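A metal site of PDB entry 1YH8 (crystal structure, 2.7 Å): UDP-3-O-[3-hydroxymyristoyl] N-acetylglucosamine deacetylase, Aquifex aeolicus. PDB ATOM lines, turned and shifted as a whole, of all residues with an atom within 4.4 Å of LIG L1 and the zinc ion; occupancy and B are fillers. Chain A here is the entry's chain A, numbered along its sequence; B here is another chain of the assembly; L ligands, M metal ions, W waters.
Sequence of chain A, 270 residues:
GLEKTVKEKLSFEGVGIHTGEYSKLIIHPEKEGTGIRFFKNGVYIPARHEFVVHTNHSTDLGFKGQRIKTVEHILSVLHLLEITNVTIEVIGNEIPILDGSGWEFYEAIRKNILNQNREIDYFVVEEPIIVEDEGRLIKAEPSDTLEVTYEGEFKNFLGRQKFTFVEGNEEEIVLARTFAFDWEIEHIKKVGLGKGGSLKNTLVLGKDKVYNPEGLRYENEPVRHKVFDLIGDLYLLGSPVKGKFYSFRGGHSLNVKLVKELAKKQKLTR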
ATOM      1  N   ILE A  17     -11.031   3.560  20.046  1.00  0.00           N
ATOM      2  CA  ILE A  17     -12.291   3.770  20.724  1.00  0.00           C
ATOM      3  C   ILE A  17     -12.916   5.133  20.416  1.00  0.00           C
ATOM      4  O   ILE A  17     -14.137   5.246  20.361  1.00  0.00           O
ATOM      5  CB  ILE A  17     -12.124   3.604  22.258  1.00  0.00           C
ATOM      6  CG1 ILE A  17     -13.509   3.509  22.903  1.00  0.00           C
ATOM      7  CG2 ILE A  17     -11.333   4.774  22.835  1.00  0.00           C
ATOM      8  CD1 ILE A  17     -13.476   3.382  24.407  1.00  0.00           C
ATOM      9  N   HIS A  18     -12.085   6.145  20.206  1.00  0.00           N
ATOM     10  CA  HIS A  18     -12.607   7.481  19.915  1.00  0.00           C
ATOM     11  C   HIS A  18     -12.750   7.826  18.437  1.00  0.00           C
ATOM     12  O   HIS A  18     -13.791   8.331  18.017  1.00  0.00           O
ATOM     13  CB  HIS A  18     -11.733   8.548  20.582  1.00  0.00           C
ATOM     14  CG  HIS A  18     -11.899   8.607  22.072  1.00  0.00           C
ATOM     15  ND1 HIS A  18     -13.125   8.807  22.678  1.00  0.00           N
ATOM     16  CD2 HIS A  18     -10.996   8.516  23.081  1.00  0.00           C
ATOM     17  CE1 HIS A  18     -12.965   8.832  23.983  1.00  0.00           C
ATOM     18  NE2 HIS A  18     -11.685   8.653  24.258  1.00  0.00           N
ATOM     19  N   HIS A  57     -11.476  12.411  28.361  1.00  0.00           N
ATOM     20  CA  HIS A  57     -11.869  11.105  27.833  1.00  0.00           C
ATOM     21  C   HIS A  57     -10.703  10.273  27.304  1.00  0.00           C
ATOM     22  O   HIS A  57     -10.907   9.148  26.828  1.00  0.00           O
ATOM     23  CB  HIS A  57     -12.933  11.295  26.750  1.00  0.00           C
ATOM     24  CG  HIS A  57     -14.040  12.212  27.174  1.00  0.00           C
ATOM     25  ND1 HIS A  57     -14.893  11.904  28.214  1.00  0.00           N
ATOM     26  CD2 HIS A  57     -14.366  13.457  26.768  1.00  0.00           C
ATOM     27  CE1 HIS A  57     -15.698  12.929  28.432  1.00  0.00           C
ATOM     28  NE2 HIS A  57     -15.394  13.888  27.566  1.00  0.00           N
ATOM     29  N   GLU A  72      -2.682   6.056  27.260  1.00  0.00           N
ATOM     30  CA  GLU A  72      -2.715   5.560  28.644  1.00  0.00           C
ATOM     31  C   GLU A  72      -2.649   4.054  28.878  1.00  0.00           C
ATOM     32  O   GLU A  72      -1.962   3.604  29.793  1.00  0.00           O
ATOM     33  CB  GLU A  72      -3.940   6.103  29.369  1.00  0.00           C
ATOM     34  CG  GLU A  72      -5.279   5.743  28.706  1.00  0.00           C
ATOM     35  CD  GLU A  72      -5.817   6.866  27.832  1.00  0.00           C
ATOM     36  OE1 GLU A  72      -5.009   7.542  27.147  1.00  0.00           O
ATOM     37  OE2 GLU A  72      -7.045   7.069  27.835  1.00  0.00           O
ATOM     38  N   HIS A  73      -3.352   3.264  28.082  1.00  0.00           N
ATOM     39  CA  HIS A  73      -3.356   1.825  28.287  1.00  0.00           C
ATOM     40  C   HIS A  73      -2.058   1.125  27.906  1.00  0.00           C
ATOM     41  O   HIS A  73      -1.586   0.256  28.638  1.00  0.00           O
ATOM     42  CB  HIS A  73      -4.544   1.193  27.550  1.00  0.00           C
ATOM     43  CG  HIS A  73      -5.881   1.629  28.080  1.00  0.00           C
ATOM     44  ND1 HIS A  73      -7.069   1.253  27.497  1.00  0.00           N
ATOM     45  CD2 HIS A  73      -6.212   2.441  29.107  1.00  0.00           C
ATOM     46  CE1 HIS A  73      -8.071   1.808  28.141  1.00  0.00           C
ATOM     47  NE2 HIS A  73      -7.579   2.535  29.125  1.00  0.00           N
ATOM     48  N   THR A 178     -12.342  -0.713  30.138  1.00  0.00           N
ATOM     49  CA  THR A 178     -12.787   0.680  30.077  1.00  0.00           C
ATOM     50  C   THR A 178     -14.284   0.721  30.366  1.00  0.00           C
ATOM     51  O   THR A 178     -15.040  -0.170  29.948  1.00  0.00           O
ATOM     52  CB  THR A 178     -12.557   1.256  28.682  1.00  0.00           C
ATOM     53  OG1 THR A 178     -11.156   1.297  28.423  1.00  0.00           O
ATOM     54  CG2 THR A 178     -13.147   2.634  28.571  1.00  0.00           C
ATOM     55  N   ILE A 185     -22.627   8.908  27.475  1.00  0.00           N
ATOM     56  CA  ILE A 185     -22.487   8.565  26.079  1.00  0.00           C
ATOM     57  C   ILE A 185     -22.962   9.597  25.078  1.00  0.00           C
ATOM     58  O   ILE A 185     -22.349   9.785  24.031  1.00  0.00           O
ATOM     59  CB  ILE A 185     -23.176   7.233  25.766  1.00  0.00           C
ATOM     60  CG1 ILE A 185     -22.538   6.111  26.597  1.00  0.00           C
ATOM     61  CG2 ILE A 185     -23.024   6.897  24.292  1.00  0.00           C
ATOM     62  CD1 ILE A 185     -23.115   4.745  26.318  1.00  0.00           C
ATOM     63  N   ILE A 188     -20.112  12.277  24.812  1.00  0.00           N
ATOM     64  CA  ILE A 188     -18.952  11.758  24.097  1.00  0.00           C
ATOM     65  C   ILE A 188     -19.185  11.796  22.591  1.00  0.00           C
ATOM     66  O   ILE A 188     -18.342  12.262  21.839  1.00  0.00           O
ATOM     67  CB  ILE A 188     -18.646  10.291  24.487  1.00  0.00           C
ATOM     68  CG1 ILE A 188     -18.528  10.163  26.004  1.00  0.00           C
ATOM     69  CG2 ILE A 188     -17.365   9.830  23.793  1.00  0.00           C
ATOM     70  CD1 ILE A 188     -17.483  11.031  26.596  1.00  0.00           C
ATOM     71  N   GLY A 194     -15.660   8.880  21.032  1.00  0.00           N
ATOM     72  CA  GLY A 194     -16.268   7.578  21.230  1.00  0.00           C
ATOM     73  C   GLY A 194     -16.827   6.912  20.002  1.00  0.00           C
ATOM     74  O   GLY A 194     -17.741   6.091  20.101  1.00  0.00           O
ATOM     75  N   GLY A 197     -16.522   3.127  20.106  1.00  0.00           N
ATOM     76  CA  GLY A 197     -17.043   2.466  21.291  1.00  0.00           C
ATOM     77  C   GLY A 197     -18.162   1.475  21.055  1.00  0.00           C
ATOM     78  O   GLY A 197     -19.022   1.665  20.204  1.00  0.00           O
ATOM     79  N   SER A 198     -18.133   0.385  21.822  1.00  0.00           N
ATOM     80  CA  SER A 198     -19.154  -0.647  21.747  1.00  0.00           C
ATOM     81  C   SER A 198     -19.085  -1.465  23.024  1.00  0.00           C
ATOM     82  O   SER A 198     -18.175  -1.291  23.829  1.00  0.00           O
ATOM     83  CB  SER A 198     -18.905  -1.554  20.549  1.00  0.00           C
ATOM     84  OG  SER A 198     -17.896  -2.504  20.844  1.00  0.00           O
ATOM     85  N   THR A 202     -16.175  -1.593  25.855  1.00  0.00           N
ATOM     86  CA  THR A 202     -16.562  -0.691  26.918  1.00  0.00           C
ATOM     87  C   THR A 202     -17.649  -1.292  27.806  1.00  0.00           C
ATOM     88  O   THR A 202     -18.585  -1.921  27.301  1.00  0.00           O
ATOM     89  CB  THR A 202     -17.133   0.643  26.369  1.00  0.00           C
ATOM     90  OG1 THR A 202     -16.209   1.243  25.448  1.00  0.00           O
ATOM     91  CG2 THR A 202     -17.401   1.616  27.509  1.00  0.00           C
ATOM     92  N   VAL A 204     -20.635  -0.504  29.778  1.00  0.00           N
ATOM     93  CA  VAL A 204     -21.596   0.567  29.919  1.00  0.00           C
ATOM     94  C   VAL A 204     -22.403   0.303  31.163  1.00  0.00           C
ATOM     95  O   VAL A 204     -23.067  -0.729  31.271  1.00  0.00           O
ATOM     96  CB  VAL A 204     -22.520   0.633  28.701  1.00  0.00           C
ATOM     97  CG1 VAL A 204     -23.475   1.811  28.850  1.00  0.00           C
ATOM     98  CG2 VAL A 204     -21.695   0.760  27.433  1.00  0.00           C
ATOM     99  N   HIS A 225      -9.769  -0.235  36.869  1.00  0.00           N
ATOM    100  CA  HIS A 225      -9.373   0.347  35.606  1.00  0.00           C
ATOM    101  C   HIS A 225      -8.853   1.746  35.846  1.00  0.00           C
ATOM    102  O   HIS A 225      -7.923   2.181  35.168  1.00  0.00           O
ATOM    103  CB  HIS A 225     -10.547   0.415  34.616  1.00  0.00           C
ATOM    104  CG  HIS A 225     -10.140   0.906  33.267  1.00  0.00           C
ATOM    105  ND1 HIS A 225      -9.505   0.087  32.350  1.00  0.00           N
ATOM    106  CD2 HIS A 225     -10.153   2.149  32.722  1.00  0.00           C
ATOM    107  CE1 HIS A 225      -9.138   0.807  31.303  1.00  0.00           C
ATOM    108  NE2 HIS A 225      -9.526   2.060  31.503  1.00  0.00           N
ATOM    109  N   ASP A 229      -5.383   3.275  34.520  1.00  0.00           N
ATOM    110  CA  ASP A 229      -5.194   4.548  33.838  1.00  0.00           C
ATOM    111  C   ASP A 229      -4.135   5.414  34.532  1.00  0.00           C
ATOM    112  O   ASP A 229      -3.176   5.876  33.899  1.00  0.00           O
ATOM    113  CB  ASP A 229      -6.508   5.329  33.760  1.00  0.00           C
ATOM    114  CG  ASP A 229      -7.455   4.796  32.687  1.00  0.00           C
ATOM    115  OD1 ASP A 229      -6.979   4.273  31.662  1.00  0.00           O
ATOM    116  OD2 ASP A 229      -8.693   4.948  32.857  1.00  0.00           O
ATOM    117  N   HIS A 252      -7.828  11.640  33.941  1.00  0.00           N
ATOM    118  CA  HIS A 252      -6.661  12.016  33.151  1.00  0.00           C
ATOM    119  C   HIS A 252      -6.151  13.434  33.382  1.00  0.00           C
ATOM    120  O   HIS A 252      -4.949  13.645  33.497  1.00  0.00           O
ATOM    121  CB  HIS A 252      -6.944  11.779  31.670  1.00  0.00           C
ATOM    122  CG  HIS A 252      -7.177  10.345  31.339  1.00  0.00           C
ATOM    123  ND1 HIS A 252      -6.265   9.354  31.658  1.00  0.00           N
ATOM    124  CD2 HIS A 252      -8.231   9.720  30.765  1.00  0.00           C
ATOM    125  CE1 HIS A 252      -6.750   8.184  31.293  1.00  0.00           C
ATOM    126  NE2 HIS A 252      -7.943   8.371  30.750  1.00  0.00           N
ATOM    127  N   ILE B 185     -32.079  -2.751  26.225  1.00  0.00           N
ATOM    128  CA  ILE B 185     -30.863  -3.358  25.710  1.00  0.00           C
ATOM    129  C   ILE B 185     -30.273  -4.469  26.548  1.00  0.00           C
ATOM    130  O   ILE B 185     -29.761  -5.450  25.997  1.00  0.00           O
ATOM    131  CB  ILE B 185     -29.786  -2.290  25.462  1.00  0.00           C
ATOM    132  CG1 ILE B 185     -30.289  -1.298  24.409  1.00  0.00           C
ATOM    133  CG2 ILE B 185     -28.530  -2.953  24.936  1.00  0.00           C
ATOM    134  CD1 ILE B 185     -29.273  -0.218  24.065  1.00  0.00           C
ATOM    135  N   VAL B 204     -31.064   4.488  19.562  1.00  0.00           N
ATOM    136  CA  VAL B 204     -31.196   4.189  20.967  1.00  0.00           C
ATOM    137  C   VAL B 204     -31.763   5.416  21.651  1.00  0.00           C
ATOM    138  O   VAL B 204     -31.187   6.499  21.592  1.00  0.00           O
ATOM    139  CB  VAL B 204     -29.843   3.829  21.589  1.00  0.00           C
ATOM    140  CG1 VAL B 204     -30.027   3.479  23.061  1.00  0.00           C
ATOM    141  CG2 VAL B 204     -29.216   2.660  20.824  1.00  0.00           C
ATOM    142  N   TYR B 211     -29.413   8.926  22.072  1.00  0.00           N
ATOM    143  CA  TYR B 211     -27.981   8.620  22.092  1.00  0.00           C
ATOM    144  C   TYR B 211     -27.298   8.894  20.750  1.00  0.00           C
ATOM    145  O   TYR B 211     -26.216   9.475  20.707  1.00  0.00           O
ATOM    146  CB  TYR B 211     -27.745   7.156  22.485  1.00  0.00           C
ATOM    147  CG  TYR B 211     -28.014   6.844  23.950  1.00  0.00           C
ATOM    148  CD1 TYR B 211     -29.321   6.711  24.422  1.00  0.00           C
ATOM    149  CD2 TYR B 211     -26.963   6.709  24.855  1.00  0.00           C
ATOM    150  CE1 TYR B 211     -29.571   6.452  25.764  1.00  0.00           C
ATOM    151  CE2 TYR B 211     -27.201   6.442  26.199  1.00  0.00           C
ATOM    152  CZ  TYR B 211     -28.510   6.311  26.649  1.00  0.00           C
ATOM    153  OH  TYR B 211     -28.765   6.069  27.989  1.00  0.00           O
HETATM  154  C1  LIG L   1     -10.081   5.329  29.154  1.00  0.00           C
HETATM  155  O1  LIG L   1      -9.011   5.783  29.678  1.00  0.00           O
HETATM  156  O2  LIG L   1     -10.525   4.140  29.413  1.00  0.00           O
HETATM  157  C2  LIG L   1     -10.843   6.288  28.158  1.00  0.00           C
HETATM  158  C3  LIG L   1     -12.130   5.727  27.509  1.00  0.00           C
HETATM  159  C4  LIG L   1     -13.475   6.359  27.959  1.00  0.00           C
HETATM  160  C5  LIG L   1     -14.347   6.760  26.755  1.00  0.00           C
HETATM  161  C6  LIG L   1     -15.376   5.699  26.301  1.00  0.00           C
HETATM  162  C7  LIG L   1     -16.189   6.180  25.100  1.00  0.00           C
HETATM  163  C8  LIG L   1     -17.631   5.705  25.146  1.00  0.00           C
HETATM  164  C9  LIG L   1     -17.931   4.428  24.357  1.00  0.00           C
HETATM  165  C10 LIG L   1     -19.392   4.349  23.928  1.00  0.00           C
HETATM  166  C11 LIG L   1     -19.946   2.941  23.913  1.00  0.00           C
HETATM  167  C12 LIG L   1     -21.296   2.890  23.212  1.00  0.00           C
HETATM  168  C13 LIG L   1     -22.212   1.813  23.786  1.00  0.00           C
HETATM  169  C14 LIG L   1     -23.769   2.139  23.696  1.00  0.00           C
HETATM  170  C15 LIG L   1     -25.253   2.050  23.881  1.00  0.00           C
HETATM  171  C16 LIG L   1     -26.174   2.532  24.828  1.00  0.00           C
HETATM  172  C1  LG2 L   2     -37.510  -4.374  14.099  1.00  0.00           C
HETATM  173  O1  LG2 L   2     -38.557  -4.870  13.568  1.00  0.00           O
HETATM  174  O2  LG2 L   2     -37.039  -3.214  13.776  1.00  0.00           O
HETATM  175  C2  LG2 L   2     -36.794  -5.252  15.184  1.00  0.00           C
HETATM  176  C3  LG2 L   2     -35.526  -4.639  15.805  1.00  0.00           C
HETATM  177  C4  LG2 L   2     -35.562  -4.378  17.315  1.00  0.00           C
HETATM  178  C5  LG2 L   2     -34.331  -4.949  18.019  1.00  0.00           C
HETATM  179  C6  LG2 L   2     -33.191  -3.959  18.194  1.00  0.00           C
HETATM  180  C7  LG2 L   2     -32.013  -4.591  18.886  1.00  0.00           C
HETATM  181  C8  LG2 L   2     -31.338  -3.599  19.815  1.00  0.00           C
HETATM  182  C9  LG2 L   2     -29.824  -3.770  19.939  1.00  0.00           C
HETATM  183  C10 LG2 L   2     -29.236  -2.779  20.941  1.00  0.00           C
HETATM  184  C11 LG2 L   2     -28.402  -1.688  20.297  1.00  0.00           C
HETATM  185  C12 LG2 L   2     -26.974  -1.762  20.809  1.00  0.00           C
HETATM  186  C13 LG2 L   2     -26.224  -0.442  20.638  1.00  0.00           C
HETATM  187  C14 LG2 L   2     -24.730  -0.490  21.137  1.00  0.00           C
HETATM  188  C15 LG2 L   2     -23.273  -0.868  21.260  1.00  0.00           C
HETATM  189  C16 LG2 L   2     -22.532  -2.048  21.093  1.00  0.00           C
HETATM  190 ZN    ZN M   1      -8.594   3.578  30.543  1.00  0.00          ZN
HETATM  191  O   HOH W   1     -13.202   4.222  31.443  1.00  0.00           O
HETATM  192  O   HOH W   2     -14.360   9.050  29.370  1.00  0.00           O
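The side-chain carboxylate (OE2) of Glu 72 lies close to an oxygen (O1) of LIG L1 (3.0 Å). Residues that only touch LIG L1: His 57, Ile 17, Gly 197, His 18, Ile 185 of chain A, Ser 198, Thr 202 and Val 204 of chain A. 14 residues have an atom within 4 Å of LIG L1: Ile 17, His 18, His 57, Glu 72, His 73, Thr 178, Ile 185 of chain A, Gly 197, Ser 198, Thr 202, Val 204 of chain A, His 225, Asp 229 and His 252. Along chain A the residues within 4 Å of LIG L1 span positions 17 to 252.
Three residues have an atom within 4 Å of the zinc ion: His 73, His 225 and Asp 229.
The zinc ion is bound by a ring nitrogen (NE2) of His 225, a ring nitrogen (NE2) of His 73, the side-chain carboxylate (OD1) of Asp 229, an oxygen (O2) of LIG L1 and an oxygen (O1) of LIG L1. The zinc ion has five donor atoms within binding distance. Slightly farther from the zinc ion lies the side-chain carboxylate (OD2) of Asp 229 (2.7 Å).
A ring nitrogen (NE2) of His 252 lies close to an oxygen (O1) of LIG L1, at 3.0 Å. The side-chain hydroxyl (OG1) of Thr 178 sits close to an oxygen (O2) of LIG L1 (3.1 Å).
O of Ile 17 is in hydrogen-bond range of N of Gly 197 (3.2 Å). A ring nitrogen (NE2) of His 252 is in hydrogen-bond range of the side-chain carboxylate of Glu 72, 3.3 Å away. The backbone carbonyl oxygen (O) of His 57 sits at hydrogen-bond distance from a ring nitrogen (NE2) of His 18 (2.7 Å). ND1 of His 18 is in hydrogen-bond range of N of Gly 194 (3.0 Å).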
